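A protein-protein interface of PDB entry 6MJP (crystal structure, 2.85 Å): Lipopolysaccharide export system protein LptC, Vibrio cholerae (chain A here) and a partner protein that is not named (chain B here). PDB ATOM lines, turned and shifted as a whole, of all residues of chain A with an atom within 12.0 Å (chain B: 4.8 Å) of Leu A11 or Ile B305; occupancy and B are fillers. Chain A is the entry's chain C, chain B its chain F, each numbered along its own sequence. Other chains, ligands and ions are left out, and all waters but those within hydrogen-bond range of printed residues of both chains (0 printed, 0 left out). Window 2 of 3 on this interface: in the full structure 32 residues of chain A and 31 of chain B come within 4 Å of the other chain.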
ATOM      1  N   SER A   2      16.652  13.902  17.559  1.00  0.00           N
ATOM      2  CA  SER A   2      16.127  12.710  18.220  1.00  0.00           C
ATOM      3  C   SER A   2      17.022  12.219  19.362  1.00  0.00           C
ATOM      4  O   SER A   2      18.190  11.913  19.142  1.00  0.00           O
ATOM      5  CB  SER A   2      15.950  11.585  17.216  1.00  0.00           C
ATOM      6  OG  SER A   2      15.597  10.407  17.912  1.00  0.00           O
ATOM      7  N   LEU A   3      16.472  12.115  20.577  1.00  0.00           N
ATOM      8  CA  LEU A   3      17.306  11.776  21.730  1.00  0.00           C
ATOM      9  C   LEU A   3      17.783  10.331  21.669  1.00  0.00           C
ATOM     10  O   LEU A   3      18.935  10.037  22.007  1.00  0.00           O
ATOM     11  CB  LEU A   3      16.548  12.036  23.033  1.00  0.00           C
ATOM     12  CG  LEU A   3      17.250  11.630  24.337  1.00  0.00           C
ATOM     13  CD1 LEU A   3      17.157  12.733  25.402  1.00  0.00           C
ATOM     14  CD2 LEU A   3      16.701  10.294  24.864  1.00  0.00           C
ATOM     15  N   SER A   4      16.912   9.414  21.248  1.00  0.00           N
ATOM     16  CA  SER A   4      17.330   8.024  21.095  1.00  0.00           C
ATOM     17  C   SER A   4      18.441   7.890  20.055  1.00  0.00           C
ATOM     18  O   SER A   4      19.437   7.194  20.287  1.00  0.00           O
ATOM     19  CB  SER A   4      16.125   7.166  20.725  1.00  0.00           C
ATOM     20  OG  SER A   4      15.448   7.732  19.620  1.00  0.00           O
ATOM     21  N   ARG A   5      18.304   8.569  18.910  1.00  0.00           N
ATOM     22  CA  ARG A   5      19.366   8.536  17.908  1.00  0.00           C
ATOM     23  C   ARG A   5      20.654   9.194  18.407  1.00  0.00           C
ATOM     24  O   ARG A   5      21.747   8.802  17.984  1.00  0.00           O
ATOM     25  CB  ARG A   5      18.889   9.203  16.617  1.00  0.00           C
ATOM     26  CG  ARG A   5      17.612   8.610  16.029  1.00  0.00           C
ATOM     27  CD  ARG A   5      17.880   7.329  15.236  1.00  0.00           C
ATOM     28  NE  ARG A   5      16.816   7.001  14.278  1.00  0.00           N
ATOM     29  CZ  ARG A   5      15.932   6.007  14.409  1.00  0.00           C
ATOM     30  NH1 ARG A   5      15.946   5.204  15.470  1.00  0.00           N
ATOM     31  NH2 ARG A   5      15.027   5.816  13.463  1.00  0.00           N
ATOM     32  N   ILE A   6      20.563  10.189  19.292  1.00  0.00           N
ATOM     33  CA  ILE A   6      21.777  10.783  19.841  1.00  0.00           C
ATOM     34  C   ILE A   6      22.490   9.783  20.732  1.00  0.00           C
ATOM     35  O   ILE A   6      23.717   9.639  20.678  1.00  0.00           O
ATOM     36  CB  ILE A   6      21.453  12.077  20.608  1.00  0.00           C
ATOM     37  CG1 ILE A   6      21.008  13.171  19.639  1.00  0.00           C
ATOM     38  CG2 ILE A   6      22.674  12.540  21.403  1.00  0.00           C
ATOM     39  CD1 ILE A   6      20.591  14.446  20.314  1.00  0.00           C
ATOM     40  N   VAL A   7      21.735   9.079  21.568  1.00  0.00           N
ATOM     41  CA  VAL A   7      22.340   8.038  22.386  1.00  0.00           C
ATOM     42  C   VAL A   7      22.924   6.931  21.506  1.00  0.00           C
ATOM     43  O   VAL A   7      24.040   6.454  21.753  1.00  0.00           O
ATOM     44  CB  VAL A   7      21.315   7.512  23.403  1.00  0.00           C
ATOM     45  CG1 VAL A   7      21.817   6.247  24.079  1.00  0.00           C
ATOM     46  CG2 VAL A   7      21.038   8.604  24.419  1.00  0.00           C
ATOM     47  N   TYR A   8      22.217   6.537  20.439  1.00  0.00           N
ATOM     48  CA  TYR A   8      22.777   5.500  19.576  1.00  0.00           C
ATOM     49  C   TYR A   8      24.112   5.944  18.987  1.00  0.00           C
ATOM     50  O   TYR A   8      25.074   5.167  18.972  1.00  0.00           O
ATOM     51  CB  TYR A   8      21.791   5.106  18.462  1.00  0.00           C
ATOM     52  CG  TYR A   8      20.483   4.508  18.959  1.00  0.00           C
ATOM     53  CD1 TYR A   8      20.416   3.825  20.173  1.00  0.00           C
ATOM     54  CD2 TYR A   8      19.311   4.650  18.226  1.00  0.00           C
ATOM     55  CE1 TYR A   8      19.216   3.300  20.642  1.00  0.00           C
ATOM     56  CE2 TYR A   8      18.099   4.124  18.688  1.00  0.00           C
ATOM     57  CZ  TYR A   8      18.058   3.450  19.899  1.00  0.00           C
ATOM     58  OH  TYR A   8      16.863   2.921  20.366  1.00  0.00           O
ATOM     59  N   VAL A   9      24.207   7.201  18.536  1.00  0.00           N
ATOM     60  CA  VAL A   9      25.474   7.693  17.990  1.00  0.00           C
ATOM     61  C   VAL A   9      26.565   7.707  19.061  1.00  0.00           C
ATOM     62  O   VAL A   9      27.692   7.263  18.811  1.00  0.00           O
ATOM     63  CB  VAL A   9      25.299   9.077  17.340  1.00  0.00           C
ATOM     64  CG1 VAL A   9      26.638   9.654  16.993  1.00  0.00           C
ATOM     65  CG2 VAL A   9      24.493   8.969  16.078  1.00  0.00           C
ATOM     66  N   LEU A  10      26.254   8.199  20.267  1.00  0.00           N
ATOM     67  CA  LEU A  10      27.219   8.118  21.357  1.00  0.00           C
ATOM     68  C   LEU A  10      27.674   6.685  21.590  1.00  0.00           C
ATOM     69  O   LEU A  10      28.868   6.433  21.780  1.00  0.00           O
ATOM     70  CB  LEU A  10      26.629   8.701  22.633  1.00  0.00           C
ATOM     71  CG  LEU A  10      26.294  10.192  22.577  1.00  0.00           C
ATOM     72  CD1 LEU A  10      25.728  10.631  23.913  1.00  0.00           C
ATOM     73  CD2 LEU A  10      27.506  11.040  22.172  1.00  0.00           C
ATOM     74  N   LEU A  11      26.735   5.730  21.581  1.00  0.00           N
ATOM     75  CA  LEU A  11      27.109   4.325  21.742  1.00  0.00           C
ATOM     76  C   LEU A  11      28.022   3.861  20.612  1.00  0.00           C
ATOM     77  O   LEU A  11      28.935   3.058  20.830  1.00  0.00           O
ATOM     78  CB  LEU A  11      25.863   3.450  21.802  1.00  0.00           C
ATOM     79  CG  LEU A  11      24.977   3.546  23.038  1.00  0.00           C
ATOM     80  CD1 LEU A  11      23.689   2.794  22.826  1.00  0.00           C
ATOM     81  CD2 LEU A  11      25.688   2.976  24.237  1.00  0.00           C
ATOM     82  N   LEU A  12      27.804   4.358  19.401  1.00  0.00           N
ATOM     83  CA  LEU A  12      28.658   3.928  18.307  1.00  0.00           C
ATOM     84  C   LEU A  12      30.055   4.506  18.459  1.00  0.00           C
ATOM     85  O   LEU A  12      31.046   3.871  18.078  1.00  0.00           O
ATOM     86  CB  LEU A  12      28.030   4.328  16.980  1.00  0.00           C
ATOM     87  CG  LEU A  12      28.609   3.724  15.712  1.00  0.00           C
ATOM     88  CD1 LEU A  12      28.846   2.231  15.873  1.00  0.00           C
ATOM     89  CD2 LEU A  12      27.588   4.000  14.651  1.00  0.00           C
ATOM     90  N   PHE A  13      30.153   5.712  19.025  1.00  0.00           N
ATOM     91  CA  PHE A  13      31.453   6.310  19.331  1.00  0.00           C
ATOM     92  C   PHE A  13      32.247   5.438  20.296  1.00  0.00           C
ATOM     93  O   PHE A  13      33.409   5.103  20.041  1.00  0.00           O
ATOM     94  CB  PHE A  13      31.260   7.703  19.936  1.00  0.00           C
ATOM     95  CG  PHE A  13      30.966   8.788  18.933  1.00  0.00           C
ATOM     96  CD1 PHE A  13      31.406   8.697  17.627  1.00  0.00           C
ATOM     97  CD2 PHE A  13      30.254   9.917  19.316  1.00  0.00           C
ATOM     98  CE1 PHE A  13      31.135   9.710  16.712  1.00  0.00           C
ATOM     99  CE2 PHE A  13      29.981  10.929  18.413  1.00  0.00           C
ATOM    100  CZ  PHE A  13      30.424  10.825  17.107  1.00  0.00           C
ATOM    101  N   ILE A  14      31.628   5.074  21.424  1.00  0.00           N
ATOM    102  CA  ILE A  14      32.299   4.258  22.429  1.00  0.00           C
ATOM    103  C   ILE A  14      32.701   2.909  21.853  1.00  0.00           C
ATOM    104  O   ILE A  14      33.776   2.383  22.166  1.00  0.00           O
ATOM    105  CB  ILE A  14      31.395   4.062  23.654  1.00  0.00           C
ATOM    106  CG1 ILE A  14      30.860   5.382  24.218  1.00  0.00           C
ATOM    107  CG2 ILE A  14      32.118   3.238  24.709  1.00  0.00           C
ATOM    108  CD1 ILE A  14      29.729   5.155  25.214  1.00  0.00           C
ATOM    109  N   ALA A  15      31.834   2.304  21.035  1.00  0.00           N
ATOM    110  CA  ALA A  15      32.151   1.000  20.455  1.00  0.00           C
ATOM    111  C   ALA A  15      33.361   1.084  19.534  1.00  0.00           C
ATOM    112  O   ALA A  15      34.318   0.316  19.682  1.00  0.00           O
ATOM    113  CB  ALA A  15      30.947   0.441  19.705  1.00  0.00           C
ATOM    114  N   SER A  16      33.336   2.018  18.575  1.00  0.00           N
ATOM    115  CA  SER A  16      34.490   2.228  17.707  1.00  0.00           C
ATOM    116  C   SER A  16      35.757   2.475  18.513  1.00  0.00           C
ATOM    117  O   SER A  16      36.816   1.907  18.210  1.00  0.00           O
ATOM    118  CB  SER A  16      34.247   3.404  16.769  1.00  0.00           C
ATOM    119  OG  SER A  16      33.187   3.161  15.866  1.00  0.00           O
ATOM    120  N   TRP A  17      35.671   3.328  19.543  1.00  0.00           N
ATOM    121  CA  TRP A  17      36.855   3.657  20.329  1.00  0.00           C
ATOM    122  C   TRP A  17      37.407   2.426  21.040  1.00  0.00           C
ATOM    123  O   TRP A  17      38.610   2.155  20.965  1.00  0.00           O
ATOM    124  CB  TRP A  17      36.555   4.777  21.327  1.00  0.00           C
ATOM    125  CG  TRP A  17      37.812   5.229  22.007  1.00  0.00           C
ATOM    126  CD1 TRP A  17      38.667   6.217  21.595  1.00  0.00           C
ATOM    127  CD2 TRP A  17      38.398   4.660  23.182  1.00  0.00           C
ATOM    128  NE1 TRP A  17      39.737   6.302  22.455  1.00  0.00           N
ATOM    129  CE2 TRP A  17      39.596   5.356  23.436  1.00  0.00           C
ATOM    130  CE3 TRP A  17      38.018   3.632  24.050  1.00  0.00           C
ATOM    131  CZ2 TRP A  17      40.413   5.058  24.524  1.00  0.00           C
ATOM    132  CZ3 TRP A  17      38.828   3.336  25.123  1.00  0.00           C
ATOM    133  CH2 TRP A  17      40.013   4.046  25.353  1.00  0.00           C
ATOM    134  N   SER A  18      36.546   1.655  21.716  1.00  0.00           N
ATOM    135  CA  SER A  18      37.007   0.424  22.360  1.00  0.00           C
ATOM    136  C   SER A  18      37.630  -0.546  21.356  1.00  0.00           C
ATOM    137  O   SER A  18      38.649  -1.180  21.654  1.00  0.00           O
ATOM    138  CB  SER A  18      35.865  -0.277  23.097  1.00  0.00           C
ATOM    139  OG  SER A  18      35.247   0.548  24.059  1.00  0.00           O
ATOM    140  N   LEU A  19      37.015  -0.718  20.181  1.00  0.00           N
ATOM    141  CA  LEU A  19      37.560  -1.691  19.238  1.00  0.00           C
ATOM    142  C   LEU A  19      38.960  -1.287  18.815  1.00  0.00           C
ATOM    143  O   LEU A  19      39.897  -2.096  18.859  1.00  0.00           O
ATOM    144  CB  LEU A  19      36.653  -1.844  18.013  1.00  0.00           C
ATOM    145  CG  LEU A  19      37.270  -2.648  16.846  1.00  0.00           C
ATOM    146  CD1 LEU A  19      37.495  -4.122  17.182  1.00  0.00           C
ATOM    147  CD2 LEU A  19      36.456  -2.524  15.574  1.00  0.00           C
ATOM    148  N   TYR A  20      39.126  -0.016  18.448  1.00  0.00           N
ATOM    149  CA  TYR A  20      40.409   0.465  17.953  1.00  0.00           C
ATOM    150  C   TYR A  20      41.441   0.599  19.068  1.00  0.00           C
ATOM    151  O   TYR A  20      42.643   0.503  18.806  1.00  0.00           O
ATOM    152  CB  TYR A  20      40.208   1.780  17.210  1.00  0.00           C
ATOM    153  CG  TYR A  20      39.614   1.574  15.836  1.00  0.00           C
ATOM    154  CD1 TYR A  20      40.320   0.885  14.859  1.00  0.00           C
ATOM    155  CD2 TYR A  20      38.352   2.056  15.510  1.00  0.00           C
ATOM    156  CE1 TYR A  20      39.795   0.685  13.595  1.00  0.00           C
ATOM    157  CE2 TYR A  20      37.810   1.858  14.236  1.00  0.00           C
ATOM    158  CZ  TYR A  20      38.541   1.172  13.286  1.00  0.00           C
ATOM    159  OH  TYR A  20      38.028   0.965  12.023  1.00  0.00           O
ATOM    160  N   TYR B  69      19.653 -12.800  25.760  1.00  0.00           N
ATOM    161  CA  TYR B  69      19.351 -11.438  25.319  1.00  0.00           C
ATOM    162  C   TYR B  69      18.436 -11.418  24.100  1.00  0.00           C
ATOM    163  O   TYR B  69      17.362 -10.807  24.123  1.00  0.00           O
ATOM    164  CB  TYR B  69      20.675 -10.733  25.015  1.00  0.00           C
ATOM    165  CG  TYR B  69      20.668  -9.243  24.709  1.00  0.00           C
ATOM    166  CD1 TYR B  69      20.484  -8.298  25.711  1.00  0.00           C
ATOM    167  CD2 TYR B  69      20.945  -8.786  23.426  1.00  0.00           C
ATOM    168  CE1 TYR B  69      20.525  -6.930  25.425  1.00  0.00           C
ATOM    169  CE2 TYR B  69      20.988  -7.436  23.133  1.00  0.00           C
ATOM    170  CZ  TYR B  69      20.779  -6.511  24.127  1.00  0.00           C
ATOM    171  OH  TYR B  69      20.831  -5.175  23.790  1.00  0.00           O
ATOM    172  N   LEU B 282      17.923  -4.587  31.156  1.00  0.00           N
ATOM    173  CA  LEU B 282      17.984  -3.516  30.169  1.00  0.00           C
ATOM    174  C   LEU B 282      17.088  -3.810  28.968  1.00  0.00           C
ATOM    175  O   LEU B 282      16.396  -2.913  28.469  1.00  0.00           O
ATOM    176  CB  LEU B 282      19.429  -3.292  29.726  1.00  0.00           C
ATOM    177  CG  LEU B 282      19.638  -2.340  28.550  1.00  0.00           C
ATOM    178  CD1 LEU B 282      19.104  -0.956  28.845  1.00  0.00           C
ATOM    179  CD2 LEU B 282      21.107  -2.273  28.235  1.00  0.00           C
ATOM    180  N   LEU B 286      13.149  -2.624  26.354  1.00  0.00           N
ATOM    181  CA  LEU B 286      13.571  -2.326  24.984  1.00  0.00           C
ATOM    182  C   LEU B 286      12.806  -3.136  23.943  1.00  0.00           C
ATOM    183  O   LEU B 286      12.747  -2.747  22.765  1.00  0.00           O
ATOM    184  CB  LEU B 286      15.081  -2.586  24.844  1.00  0.00           C
ATOM    185  CG  LEU B 286      15.760  -2.418  23.477  1.00  0.00           C
ATOM    186  CD1 LEU B 286      15.604  -0.997  22.972  1.00  0.00           C
ATOM    187  CD2 LEU B 286      17.226  -2.805  23.534  1.00  0.00           C
ATOM    188  N   PRO B 301      19.469  -1.400  17.446  1.00  0.00           N
ATOM    189  CA  PRO B 301      19.818  -0.849  18.763  1.00  0.00           C
ATOM    190  C   PRO B 301      20.247  -1.892  19.778  1.00  0.00           C
ATOM    191  O   PRO B 301      21.172  -1.634  20.557  1.00  0.00           O
ATOM    192  CB  PRO B 301      18.522  -0.147  19.194  1.00  0.00           C
ATOM    193  CG  PRO B 301      17.838   0.177  17.932  1.00  0.00           C
ATOM    194  CD  PRO B 301      18.132  -0.964  17.012  1.00  0.00           C
ATOM    195  N   ALA B 302      19.605  -3.063  19.801  1.00  0.00           N
ATOM    196  CA  ALA B 302      19.941  -4.059  20.818  1.00  0.00           C
ATOM    197  C   ALA B 302      21.339  -4.626  20.611  1.00  0.00           C
ATOM    198  O   ALA B 302      22.085  -4.826  21.576  1.00  0.00           O
ATOM    199  CB  ALA B 302      18.910  -5.183  20.817  1.00  0.00           C
ATOM    200  N   ILE B 303      21.697  -4.919  19.357  1.00  0.00           N
ATOM    201  CA  ILE B 303      23.012  -5.465  19.065  1.00  0.00           C
ATOM    202  C   ILE B 303      24.067  -4.389  19.258  1.00  0.00           C
ATOM    203  O   ILE B 303      25.157  -4.661  19.776  1.00  0.00           O
ATOM    204  CB  ILE B 303      23.002  -6.074  17.644  1.00  0.00           C
ATOM    205  CG1 ILE B 303      22.151  -7.352  17.655  1.00  0.00           C
ATOM    206  CG2 ILE B 303      24.417  -6.363  17.112  1.00  0.00           C
ATOM    207  CD1 ILE B 303      22.228  -8.167  16.390  1.00  0.00           C
ATOM    208  N   LEU B 304      23.742  -3.145  18.905  1.00  0.00           N
ATOM    209  CA  LEU B 304      24.652  -2.031  19.153  1.00  0.00           C
ATOM    210  C   LEU B 304      24.976  -1.885  20.637  1.00  0.00           C
ATOM    211  O   LEU B 304      26.123  -1.613  21.007  1.00  0.00           O
ATOM    212  CB  LEU B 304      24.032  -0.754  18.609  1.00  0.00           C
ATOM    213  CG  LEU B 304      24.746   0.533  18.931  1.00  0.00           C
ATOM    214  CD1 LEU B 304      26.107   0.504  18.257  1.00  0.00           C
ATOM    215  CD2 LEU B 304      23.888   1.688  18.440  1.00  0.00           C
ATOM    216  N   ILE B 305      23.980  -2.079  21.496  1.00  0.00           N
ATOM    217  CA  ILE B 305      24.171  -1.962  22.938  1.00  0.00           C
ATOM    218  C   ILE B 305      25.067  -3.078  23.450  1.00  0.00           C
ATOM    219  O   ILE B 305      25.932  -2.863  24.312  1.00  0.00           O
ATOM    220  CB  ILE B 305      22.802  -1.989  23.639  1.00  0.00           C
ATOM    221  CG1 ILE B 305      22.081  -0.653  23.455  1.00  0.00           C
ATOM    222  CG2 ILE B 305      22.929  -2.422  25.103  1.00  0.00           C
ATOM    223  CD1 ILE B 305      20.670  -0.689  23.935  1.00  0.00           C
ATOM    224  N   TYR B 306      24.833  -4.300  22.959  1.00  0.00           N
ATOM    225  CA  TYR B 306      25.636  -5.456  23.350  1.00  0.00           C
ATOM    226  C   TYR B 306      27.078  -5.300  22.897  1.00  0.00           C
ATOM    227  O   TYR B 306      28.013  -5.658  23.622  1.00  0.00           O
ATOM    228  CB  TYR B 306      25.029  -6.717  22.744  1.00  0.00           C
ATOM    229  CG  TYR B 306      25.656  -8.039  23.167  1.00  0.00           C
ATOM    230  CD1 TYR B 306      26.823  -8.515  22.569  1.00  0.00           C
ATOM    231  CD2 TYR B 306      25.052  -8.838  24.134  1.00  0.00           C
ATOM    232  CE1 TYR B 306      27.382  -9.730  22.951  1.00  0.00           C
ATOM    233  CE2 TYR B 306      25.602 -10.050  24.520  1.00  0.00           C
ATOM    234  CZ  TYR B 306      26.766 -10.493  23.923  1.00  0.00           C
ATOM    235  OH  TYR B 306      27.315 -11.702  24.305  1.00  0.00           O
ATOM    236  N   LEU B 307      27.277  -4.803  21.677  1.00  0.00           N
ATOM    237  CA  LEU B 307      28.632  -4.628  21.183  1.00  0.00           C
ATOM    238  C   LEU B 307      29.369  -3.591  22.015  1.00  0.00           C
ATOM    239  O   LEU B 307      30.498  -3.830  22.457  1.00  0.00           O
ATOM    240  CB  LEU B 307      28.612  -4.246  19.702  1.00  0.00           C
ATOM    241  CG  LEU B 307      28.791  -5.382  18.683  1.00  0.00           C
ATOM    242  CD1 LEU B 307      27.831  -6.543  18.959  1.00  0.00           C
ATOM    243  CD2 LEU B 307      28.635  -4.868  17.243  1.00  0.00           C
ATOM    244  N   THR B 308      28.732  -2.439  22.272  1.00  0.00           N
ATOM    245  CA  THR B 308      29.405  -1.384  23.036  1.00  0.00           C
ATOM    246  C   THR B 308      29.795  -1.874  24.420  1.00  0.00           C
ATOM    247  O   THR B 308      30.882  -1.562  24.925  1.00  0.00           O
ATOM    248  CB  THR B 308      28.527  -0.142  23.174  1.00  0.00           C
ATOM    249  OG1 THR B 308      27.317  -0.497  23.851  1.00  0.00           O
ATOM    250  CG2 THR B 308      28.198   0.429  21.837  1.00  0.00           C
ATOM    251  N   TYR B 309      28.907  -2.626  25.063  1.00  0.00           N
ATOM    252  CA  TYR B 309      29.215  -3.104  26.401  1.00  0.00           C
ATOM    253  C   TYR B 309      30.423  -4.027  26.395  1.00  0.00           C
ATOM    254  O   TYR B 309      31.360  -3.840  27.177  1.00  0.00           O
ATOM    255  CB  TYR B 309      28.012  -3.818  26.993  1.00  0.00           C
ATOM    256  CG  TYR B 309      28.326  -4.450  28.320  1.00  0.00           C
ATOM    257  CD1 TYR B 309      28.480  -3.676  29.463  1.00  0.00           C
ATOM    258  CD2 TYR B 309      28.470  -5.823  28.433  1.00  0.00           C
ATOM    259  CE1 TYR B 309      28.765  -4.255  30.684  1.00  0.00           C
ATOM    260  CE2 TYR B 309      28.750  -6.414  29.642  1.00  0.00           C
ATOM    261  CZ  TYR B 309      28.898  -5.627  30.768  1.00  0.00           C
ATOM    262  OH  TYR B 309      29.173  -6.225  31.978  1.00  0.00           O
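Among the printed residues, merely in contact across the chains: Leu A11 with Thr B308 (2.9 Å), Ala A15 with Thr B308 (3.5 Å), Tyr A8 with Pro B301 (3.7 Å), Tyr A8 with Leu B304 (3.7 Å) and Leu A11 with Ile B305 (3.9 Å).
O of Leu B304 lies close to OG1 of Thr B308 (3.3 Å). OG1 of Thr B308 is in hydrogen-bond range of O of Ile B305 (2.8 Å).
Ser A4 touches none of the printed residues of chain B. Of the printed residues of chain B, Tyr A8 touches Pro B301 (3.7 Å) and Leu B304 (3.7 Å). Leu A11 touches just these residues of chain B: Ile B305 and Thr B308. Of the printed residues of chain B, Ala A15 touches Thr B308. Pro B301 touches one residue of chain A. Of the printed residues of chain A, Leu B304 touches Tyr A8 (3.7 Å). Ile B305 touches just one residue of chain A: Leu A11 (3.9 Å). No residue of chain A comes within 4 Å of Leu B307. The nearest residue of chain B that does not touch Leu A11 is Leu B304 (4.2 Å). The nearest residue of chain A that does not touch Ile B305 is Tyr A8 (5.4 Å).
Printed residues of chain B that touch a printed residue of chain A: Pro B301, Leu B304, Ile B305 and Thr B308. Printed residues of chain A that touch a printed residue of chain B: Tyr A8, Leu A11 and Ala A15. Among the printed residues, 5 pairs touch across the chains. Among the printed residues, no Asp or Glu carboxylate lies within 4 Å of a Lys or Arg side-chain nitrogen of the other chain.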
